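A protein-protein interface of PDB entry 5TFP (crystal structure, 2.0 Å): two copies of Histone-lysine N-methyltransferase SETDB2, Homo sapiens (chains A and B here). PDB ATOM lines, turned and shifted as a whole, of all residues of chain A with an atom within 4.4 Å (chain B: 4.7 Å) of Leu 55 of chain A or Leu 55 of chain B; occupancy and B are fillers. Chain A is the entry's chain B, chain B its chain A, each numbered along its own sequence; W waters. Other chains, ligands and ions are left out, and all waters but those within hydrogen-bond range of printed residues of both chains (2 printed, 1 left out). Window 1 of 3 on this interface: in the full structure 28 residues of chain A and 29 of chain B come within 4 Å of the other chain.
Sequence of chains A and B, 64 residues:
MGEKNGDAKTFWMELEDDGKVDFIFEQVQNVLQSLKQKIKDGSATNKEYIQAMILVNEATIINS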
ATOM      1  N   LEU A  32     -24.953   6.681 -27.323  1.00  0.00           N
ATOM      2  CA  LEU A  32     -24.467   7.894 -26.647  1.00  0.00           C
ATOM      3  C   LEU A  32     -25.318   9.126 -26.963  1.00  0.00           C
ATOM      4  O   LEU A  32     -25.608   9.935 -26.079  1.00  0.00           O
ATOM      5  CB  LEU A  32     -22.999   8.187 -27.021  1.00  0.00           C
ATOM      6  CG  LEU A  32     -21.978   7.221 -26.401  1.00  0.00           C
ATOM      7  CD1 LEU A  32     -20.698   7.410 -27.138  1.00  0.00           C
ATOM      8  CD2 LEU A  32     -21.758   7.490 -24.894  1.00  0.00           C
ATOM      9  N   LEU A  35     -28.538   8.822 -25.029  1.00  0.00           N
ATOM     10  CA  LEU A  35     -28.325   9.096 -23.594  1.00  0.00           C
ATOM     11  C   LEU A  35     -28.145  10.581 -23.349  1.00  0.00           C
ATOM     12  O   LEU A  35     -28.695  11.141 -22.402  1.00  0.00           O
ATOM     13  CB  LEU A  35     -27.099   8.345 -23.058  1.00  0.00           C
ATOM     14  CG  LEU A  35     -27.308   6.823 -22.933  1.00  0.00           C
ATOM     15  CD1 LEU A  35     -25.972   6.126 -22.620  1.00  0.00           C
ATOM     16  CD2 LEU A  35     -28.343   6.507 -21.863  1.00  0.00           C
ATOM     17  N   GLN A  51     -25.868   4.119 -16.720  1.00  0.00           N
ATOM     18  CA  GLN A  51     -25.178   3.705 -17.940  1.00  0.00           C
ATOM     19  C   GLN A  51     -24.310   4.823 -18.538  1.00  0.00           C
ATOM     20  O   GLN A  51     -23.152   4.599 -18.916  1.00  0.00           O
ATOM     21  CB  GLN A  51     -26.202   3.202 -18.975  1.00  0.00           C
ATOM     22  CG  GLN A  51     -25.582   2.780 -20.305  1.00  0.00           C
ATOM     23  CD  GLN A  51     -26.620   2.366 -21.313  1.00  0.00           C
ATOM     24  OE1 GLN A  51     -27.757   2.833 -21.253  1.00  0.00           O
ATOM     25  NE2 GLN A  51     -26.255   1.464 -22.228  1.00  0.00           N
ATOM     26  N   ALA A  52     -24.849   6.032 -18.637  1.00  0.00           N
ATOM     27  CA  ALA A  52     -24.075   7.146 -19.192  1.00  0.00           C
ATOM     28  C   ALA A  52     -22.846   7.526 -18.338  1.00  0.00           C
ATOM     29  O   ALA A  52     -21.765   7.799 -18.867  1.00  0.00           O
ATOM     30  CB  ALA A  52     -24.990   8.388 -19.376  1.00  0.00           C
ATOM     31  N   MET A  53     -23.014   7.546 -17.025  1.00  0.00           N
ATOM     32  CA  MET A  53     -21.902   7.796 -16.120  1.00  0.00           C
ATOM     33  C   MET A  53     -20.790   6.789 -16.315  1.00  0.00           C
ATOM     34  O   MET A  53     -19.614   7.147 -16.404  1.00  0.00           O
ATOM     35  CB  MET A  53     -22.368   7.758 -14.658  1.00  0.00           C
ATOM     36  CG  MET A  53     -21.266   8.144 -13.699  1.00  0.00           C
ATOM     37  SD  MET A  53     -21.897   8.065 -11.883  1.00  0.00           S
ATOM     38  CE  MET A  53     -22.369   6.189 -11.822  1.00  0.00           C
ATOM     39  N   ILE A  54     -21.164   5.516 -16.392  1.00  0.00           N
ATOM     40  CA  ILE A  54     -20.171   4.465 -16.537  1.00  0.00           C
ATOM     41  C   ILE A  54     -19.457   4.585 -17.878  1.00  0.00           C
ATOM     42  O   ILE A  54     -18.252   4.425 -17.941  1.00  0.00           O
ATOM     43  CB  ILE A  54     -20.824   3.070 -16.382  1.00  0.00           C
ATOM     44  CG1 ILE A  54     -21.160   2.848 -14.894  1.00  0.00           C
ATOM     45  CG2 ILE A  54     -19.893   1.981 -16.895  1.00  0.00           C
ATOM     46  CD1 ILE A  54     -21.935   1.585 -14.614  1.00  0.00           C
ATOM     47  N   LEU A  55     -20.190   4.895 -18.948  1.00  0.00           N
ATOM     48  CA  LEU A  55     -19.548   5.074 -20.269  1.00  0.00           C
ATOM     49  C   LEU A  55     -18.548   6.228 -20.302  1.00  0.00           C
ATOM     50  O   LEU A  55     -17.446   6.096 -20.873  1.00  0.00           O
ATOM     51  CB  LEU A  55     -20.607   5.305 -21.362  1.00  0.00           C
ATOM     52  CG  LEU A  55     -21.374   4.079 -21.861  1.00  0.00           C
ATOM     53  CD1 LEU A  55     -22.669   4.513 -22.583  1.00  0.00           C
ATOM     54  CD2 LEU A  55     -20.501   3.199 -22.786  1.00  0.00           C
ATOM     55  N   VAL A  56     -18.942   7.356 -19.715  1.00  0.00           N
ATOM     56  CA  VAL A  56     -18.087   8.539 -19.634  1.00  0.00           C
ATOM     57  C   VAL A  56     -16.796   8.236 -18.911  1.00  0.00           C
ATOM     58  O   VAL A  56     -15.698   8.583 -19.365  1.00  0.00           O
ATOM     59  CB  VAL A  56     -18.790   9.702 -18.905  1.00  0.00           C
ATOM     60  CG1 VAL A  56     -17.767  10.705 -18.380  1.00  0.00           C
ATOM     61  CG2 VAL A  56     -19.768  10.368 -19.830  1.00  0.00           C
ATOM     62  N   ASN A  57     -16.935   7.570 -17.775  1.00  0.00           N
ATOM     63  CA  ASN A  57     -15.784   7.263 -16.954  1.00  0.00           C
ATOM     64  C   ASN A  57     -14.871   6.230 -17.604  1.00  0.00           C
ATOM     65  O   ASN A  57     -13.666   6.255 -17.370  1.00  0.00           O
ATOM     66  CB  ASN A  57     -16.229   6.833 -15.557  1.00  0.00           C
ATOM     67  CG  ASN A  57     -16.623   8.038 -14.695  1.00  0.00           C
ATOM     68  OD1 ASN A  57     -15.765   8.807 -14.268  1.00  0.00           O
ATOM     69  ND2 ASN A  57     -17.915   8.226 -14.478  1.00  0.00           N
ATOM     70  N   GLU A  58     -15.422   5.357 -18.451  1.00  0.00           N
ATOM     71  CA  GLU A  58     -14.606   4.376 -19.163  1.00  0.00           C
ATOM     72  C   GLU A  58     -13.835   5.007 -20.328  1.00  0.00           C
ATOM     73  O   GLU A  58     -12.753   4.544 -20.684  1.00  0.00           O
ATOM     74  CB  GLU A  58     -15.472   3.241 -19.698  1.00  0.00           C
ATOM     75  CG  GLU A  58     -14.724   2.232 -20.554  1.00  0.00           C
ATOM     76  CD  GLU A  58     -13.553   1.560 -19.821  1.00  0.00           C
ATOM     77  OE1 GLU A  58     -13.657   1.345 -18.591  1.00  0.00           O
ATOM     78  OE2 GLU A  58     -12.522   1.244 -20.469  1.00  0.00           O
ATOM     79  N   ALA A  59     -14.411   6.044 -20.927  1.00  0.00           N
ATOM     80  CA  ALA A  59     -13.785   6.733 -22.064  1.00  0.00           C
ATOM     81  C   ALA A  59     -12.756   7.794 -21.655  1.00  0.00           C
ATOM     82  O   ALA A  59     -11.754   7.996 -22.347  1.00  0.00           O
ATOM     83  CB  ALA A  59     -14.861   7.381 -22.918  1.00  0.00           C
ATOM     84  N   LEU B  32     -13.860   7.696 -28.791  1.00  0.00           N
ATOM     85  CA  LEU B  32     -14.395   6.669 -29.669  1.00  0.00           C
ATOM     86  C   LEU B  32     -13.878   6.703 -31.094  1.00  0.00           C
ATOM     87  O   LEU B  32     -13.629   5.657 -31.692  1.00  0.00           O
ATOM     88  CB  LEU B  32     -15.922   6.775 -29.761  1.00  0.00           C
ATOM     89  CG  LEU B  32     -16.788   6.033 -28.763  1.00  0.00           C
ATOM     90  CD1 LEU B  32     -18.205   6.137 -29.283  1.00  0.00           C
ATOM     91  CD2 LEU B  32     -16.347   4.589 -28.629  1.00  0.00           C
ATOM     92  N   LEU B  35     -10.251   5.515 -31.095  1.00  0.00           N
ATOM     93  CA  LEU B  35     -10.156   4.076 -30.912  1.00  0.00           C
ATOM     94  C   LEU B  35     -10.542   3.365 -32.185  1.00  0.00           C
ATOM     95  O   LEU B  35      -9.885   2.424 -32.610  1.00  0.00           O
ATOM     96  CB  LEU B  35     -11.072   3.594 -29.774  1.00  0.00           C
ATOM     97  CG  LEU B  35     -10.622   3.897 -28.354  1.00  0.00           C
ATOM     98  CD1 LEU B  35     -11.713   3.502 -27.335  1.00  0.00           C
ATOM     99  CD2 LEU B  35      -9.353   3.137 -28.061  1.00  0.00           C
ATOM    100  N   GLN B  51     -10.403  -1.497 -23.933  1.00  0.00           N
ATOM    101  CA  GLN B  51     -11.217  -0.316 -23.664  1.00  0.00           C
ATOM    102  C   GLN B  51     -12.362  -0.184 -24.666  1.00  0.00           C
ATOM    103  O   GLN B  51     -13.502   0.121 -24.282  1.00  0.00           O
ATOM    104  CB  GLN B  51     -10.371   0.975 -23.702  1.00  0.00           C
ATOM    105  CG  GLN B  51     -11.184   2.259 -23.360  1.00  0.00           C
ATOM    106  CD  GLN B  51     -10.381   3.530 -23.529  1.00  0.00           C
ATOM    107  OE1 GLN B  51      -9.428   3.553 -24.308  1.00  0.00           O
ATOM    108  NE2 GLN B  51     -10.733   4.580 -22.783  1.00  0.00           N
ATOM    109  N   ALA B  52     -12.050  -0.384 -25.944  1.00  0.00           N
ATOM    110  CA  ALA B  52     -13.068  -0.297 -26.994  1.00  0.00           C
ATOM    111  C   ALA B  52     -14.139  -1.359 -26.768  1.00  0.00           C
ATOM    112  O   ALA B  52     -15.333  -1.090 -26.854  1.00  0.00           O
ATOM    113  CB  ALA B  52     -12.424  -0.449 -28.396  1.00  0.00           C
ATOM    114  N   MET B  53     -13.705  -2.572 -26.454  1.00  0.00           N
ATOM    115  CA  MET B  53     -14.663  -3.628 -26.161  1.00  0.00           C
ATOM    116  C   MET B  53     -15.556  -3.324 -24.952  1.00  0.00           C
ATOM    117  O   MET B  53     -16.763  -3.607 -24.968  1.00  0.00           O
ATOM    118  CB  MET B  53     -13.926  -4.929 -25.911  1.00  0.00           C
ATOM    119  CG  MET B  53     -14.839  -6.027 -25.571  1.00  0.00           C
ATOM    120  SD  MET B  53     -13.786  -7.624 -25.313  1.00  0.00           S
ATOM    121  CE  MET B  53     -13.091  -7.933 -27.087  1.00  0.00           C
ATOM    122  N   ILE B  54     -14.962  -2.786 -23.895  1.00  0.00           N
ATOM    123  CA  ILE B  54     -15.728  -2.419 -22.683  1.00  0.00           C
ATOM    124  C   ILE B  54     -16.776  -1.354 -23.019  1.00  0.00           C
ATOM    125  O   ILE B  54     -17.940  -1.435 -22.596  1.00  0.00           O
ATOM    126  CB  ILE B  54     -14.812  -1.913 -21.558  1.00  0.00           C
ATOM    127  CG1 ILE B  54     -13.942  -3.069 -21.034  1.00  0.00           C
ATOM    128  CG2 ILE B  54     -15.629  -1.319 -20.389  1.00  0.00           C
ATOM    129  CD1 ILE B  54     -12.868  -2.619 -20.052  1.00  0.00           C
ATOM    130  N   LEU B  55     -16.373  -0.348 -23.784  1.00  0.00           N
ATOM    131  CA  LEU B  55     -17.345   0.680 -24.224  1.00  0.00           C
ATOM    132  C   LEU B  55     -18.494   0.087 -25.048  1.00  0.00           C
ATOM    133  O   LEU B  55     -19.667   0.428 -24.844  1.00  0.00           O
ATOM    134  CB  LEU B  55     -16.628   1.782 -25.026  1.00  0.00           C
ATOM    135  CG  LEU B  55     -15.731   2.716 -24.217  1.00  0.00           C
ATOM    136  CD1 LEU B  55     -14.869   3.540 -25.166  1.00  0.00           C
ATOM    137  CD2 LEU B  55     -16.616   3.641 -23.315  1.00  0.00           C
ATOM    138  N   VAL B  56     -18.177  -0.803 -25.973  1.00  0.00           N
ATOM    139  CA  VAL B  56     -19.210  -1.456 -26.762  1.00  0.00           C
ATOM    140  C   VAL B  56     -20.226  -2.198 -25.898  1.00  0.00           C
ATOM    141  O   VAL B  56     -21.450  -2.104 -26.118  1.00  0.00           O
ATOM    142  CB  VAL B  56     -18.602  -2.475 -27.772  1.00  0.00           C
ATOM    143  CG1 VAL B  56     -19.703  -3.375 -28.306  1.00  0.00           C
ATOM    144  CG2 VAL B  56     -17.927  -1.744 -28.923  1.00  0.00           C
ATOM    145  N   ASN B  57     -19.737  -2.911 -24.888  1.00  0.00           N
ATOM    146  CA  ASN B  57     -20.624  -3.714 -24.074  1.00  0.00           C
ATOM    147  C   ASN B  57     -21.439  -2.845 -23.108  1.00  0.00           C
ATOM    148  O   ASN B  57     -22.623  -3.112 -22.893  1.00  0.00           O
ATOM    149  CB  ASN B  57     -19.834  -4.779 -23.321  1.00  0.00           C
ATOM    150  CG  ASN B  57     -19.178  -5.779 -24.262  1.00  0.00           C
ATOM    151  OD1 ASN B  57     -18.129  -6.328 -23.960  1.00  0.00           O
ATOM    152  ND2 ASN B  57     -19.782  -5.982 -25.436  1.00  0.00           N
ATOM    153  N   GLU B  58     -20.811  -1.806 -22.558  1.00  0.00           N
ATOM    154  CA  GLU B  58     -21.513  -0.867 -21.682  1.00  0.00           C
ATOM    155  C   GLU B  58     -22.580  -0.091 -22.461  1.00  0.00           C
ATOM    156  O   GLU B  58     -23.610   0.279 -21.915  1.00  0.00           O
ATOM    157  CB  GLU B  58     -20.518   0.084 -21.009  1.00  0.00           C
ATOM    158  CG  GLU B  58     -19.729  -0.635 -19.912  1.00  0.00           C
ATOM    159  CD  GLU B  58     -18.543   0.138 -19.379  1.00  0.00           C
ATOM    160  OE1 GLU B  58     -18.137   1.159 -19.994  1.00  0.00           O
ATOM    161  OE2 GLU B  58     -18.025  -0.288 -18.317  1.00  0.00           O
ATOM    162  N   ALA B  59     -22.346   0.134 -23.749  1.00  0.00           N
ATOM    163  CA  ALA B  59     -23.321   0.854 -24.538  1.00  0.00           C
ATOM    164  C   ALA B  59     -24.418  -0.085 -25.072  1.00  0.00           C
ATOM    165  O   ALA B  59     -25.582   0.310 -25.113  1.00  0.00           O
ATOM    166  CB  ALA B  59     -22.640   1.602 -25.715  1.00  0.00           C
HETATM  167  O   HOH W   1     -15.968   0.461 -17.187  1.00  0.00           O
HETATM  168  O   HOH W   2     -28.336   0.158 -24.577  1.00  0.00           O
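Ala 52 of chain A touches none of the printed residues of chain B. Of the printed residues of chain B, Leu 55 of chain A touches Leu 55 (3.6 Å), Glu 58 (3.6 Å) and Ala 59 (3.7 Å). Val 56 of chain A touches none of the printed residues of chain B. Of the printed residues of chain B, Glu 58 of chain A touches Gln 51 (2.9 Å), Ile 54 (3.6 Å), Leu 55 (3.6 Å) and Glu 58 (3.4 Å). Printed residues of chain A within 4 Å of Gln 51 of chain B: Glu 58 (2.9 Å) and Ala 59 (3.6 Å). Of chain A, only Leu 55 (3.6 Å) and Glu 58 (3.6 Å) come within 4 Å of Leu 55 of chain B. The nearest printed residue of chain B that does not touch Leu 55 of chain A is Ile 54 of chain B (5.3 Å).
Of the 11 printed residues of chain B, 6 touch a printed residue of chain A. Along chain B the printed residues that touch a printed residue of chain A span positions 32 to 59. Among the printed residues, 12 pairs touch across the chains. Among the printed residues, no Asp or Glu carboxylate lies within 4 Å of a Lys or Arg side-chain nitrogen of the other chain.
Among the printed residues, merely in contact across the chains: Ile 54 of chain A with Glu 58 of chain B, Glu 58 of chain A with Glu 58 of chain B, Leu 32 of chain A with Leu 32 of chain B, Leu 55 of chain A with Leu 55 of chain B, Leu 55 of chain A with Glu 58 of chain B, Ala 59 of chain A with Gln 51 of chain B, Glu 58 of chain A with Ile 54 of chain B, Glu 58 of chain A with Leu 55 of chain B and Leu 55 of chain A with Ala 59 of chain B.
Leu 32 of chain A touches its own counterpart, Leu 32 of chain B. Leu 55 of chain A touches its own counterpart, Leu 55 of chain B. Leu 55 of chain A touches Ala 59 of chain B, but with the chains exchanged Ala 59 of chain A does not touch Leu 55 of chain B (4.04 Å). Glu 58 of chain B touches its own counterpart, Glu 58 of chain A. Of the 12 pairs that touch across the chains among the printed residues, 11 have their exchanged pair printed and touching as well.
Water W1 bridges OE2 of Glu 58 of chain B (2.5 Å) and OE1 of Glu 58 of chain A (2.8 Å). Water W2 bridges the backbone carbonyl oxygen (O) of Ala 59 of chain B (2.8 Å) and the side-chain amide nitrogen (NE2) of Gln 51 of chain A (3.4 Å).
The backbone carbonyl oxygen (O) of Glu 58 of chain A is in hydrogen-bond range of the side-chain amide nitrogen (NE2) of Gln 51 of chain B, 2.9 Å away. O of Ala 59 of chain B sits at hydrogen-bond distance from NE2 of Gln 51 of chain A (3.2 Å). O of Glu 58 of chain B lies within hydrogen-bond range of NE2 of Gln 51 of chain A (2.9 Å).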
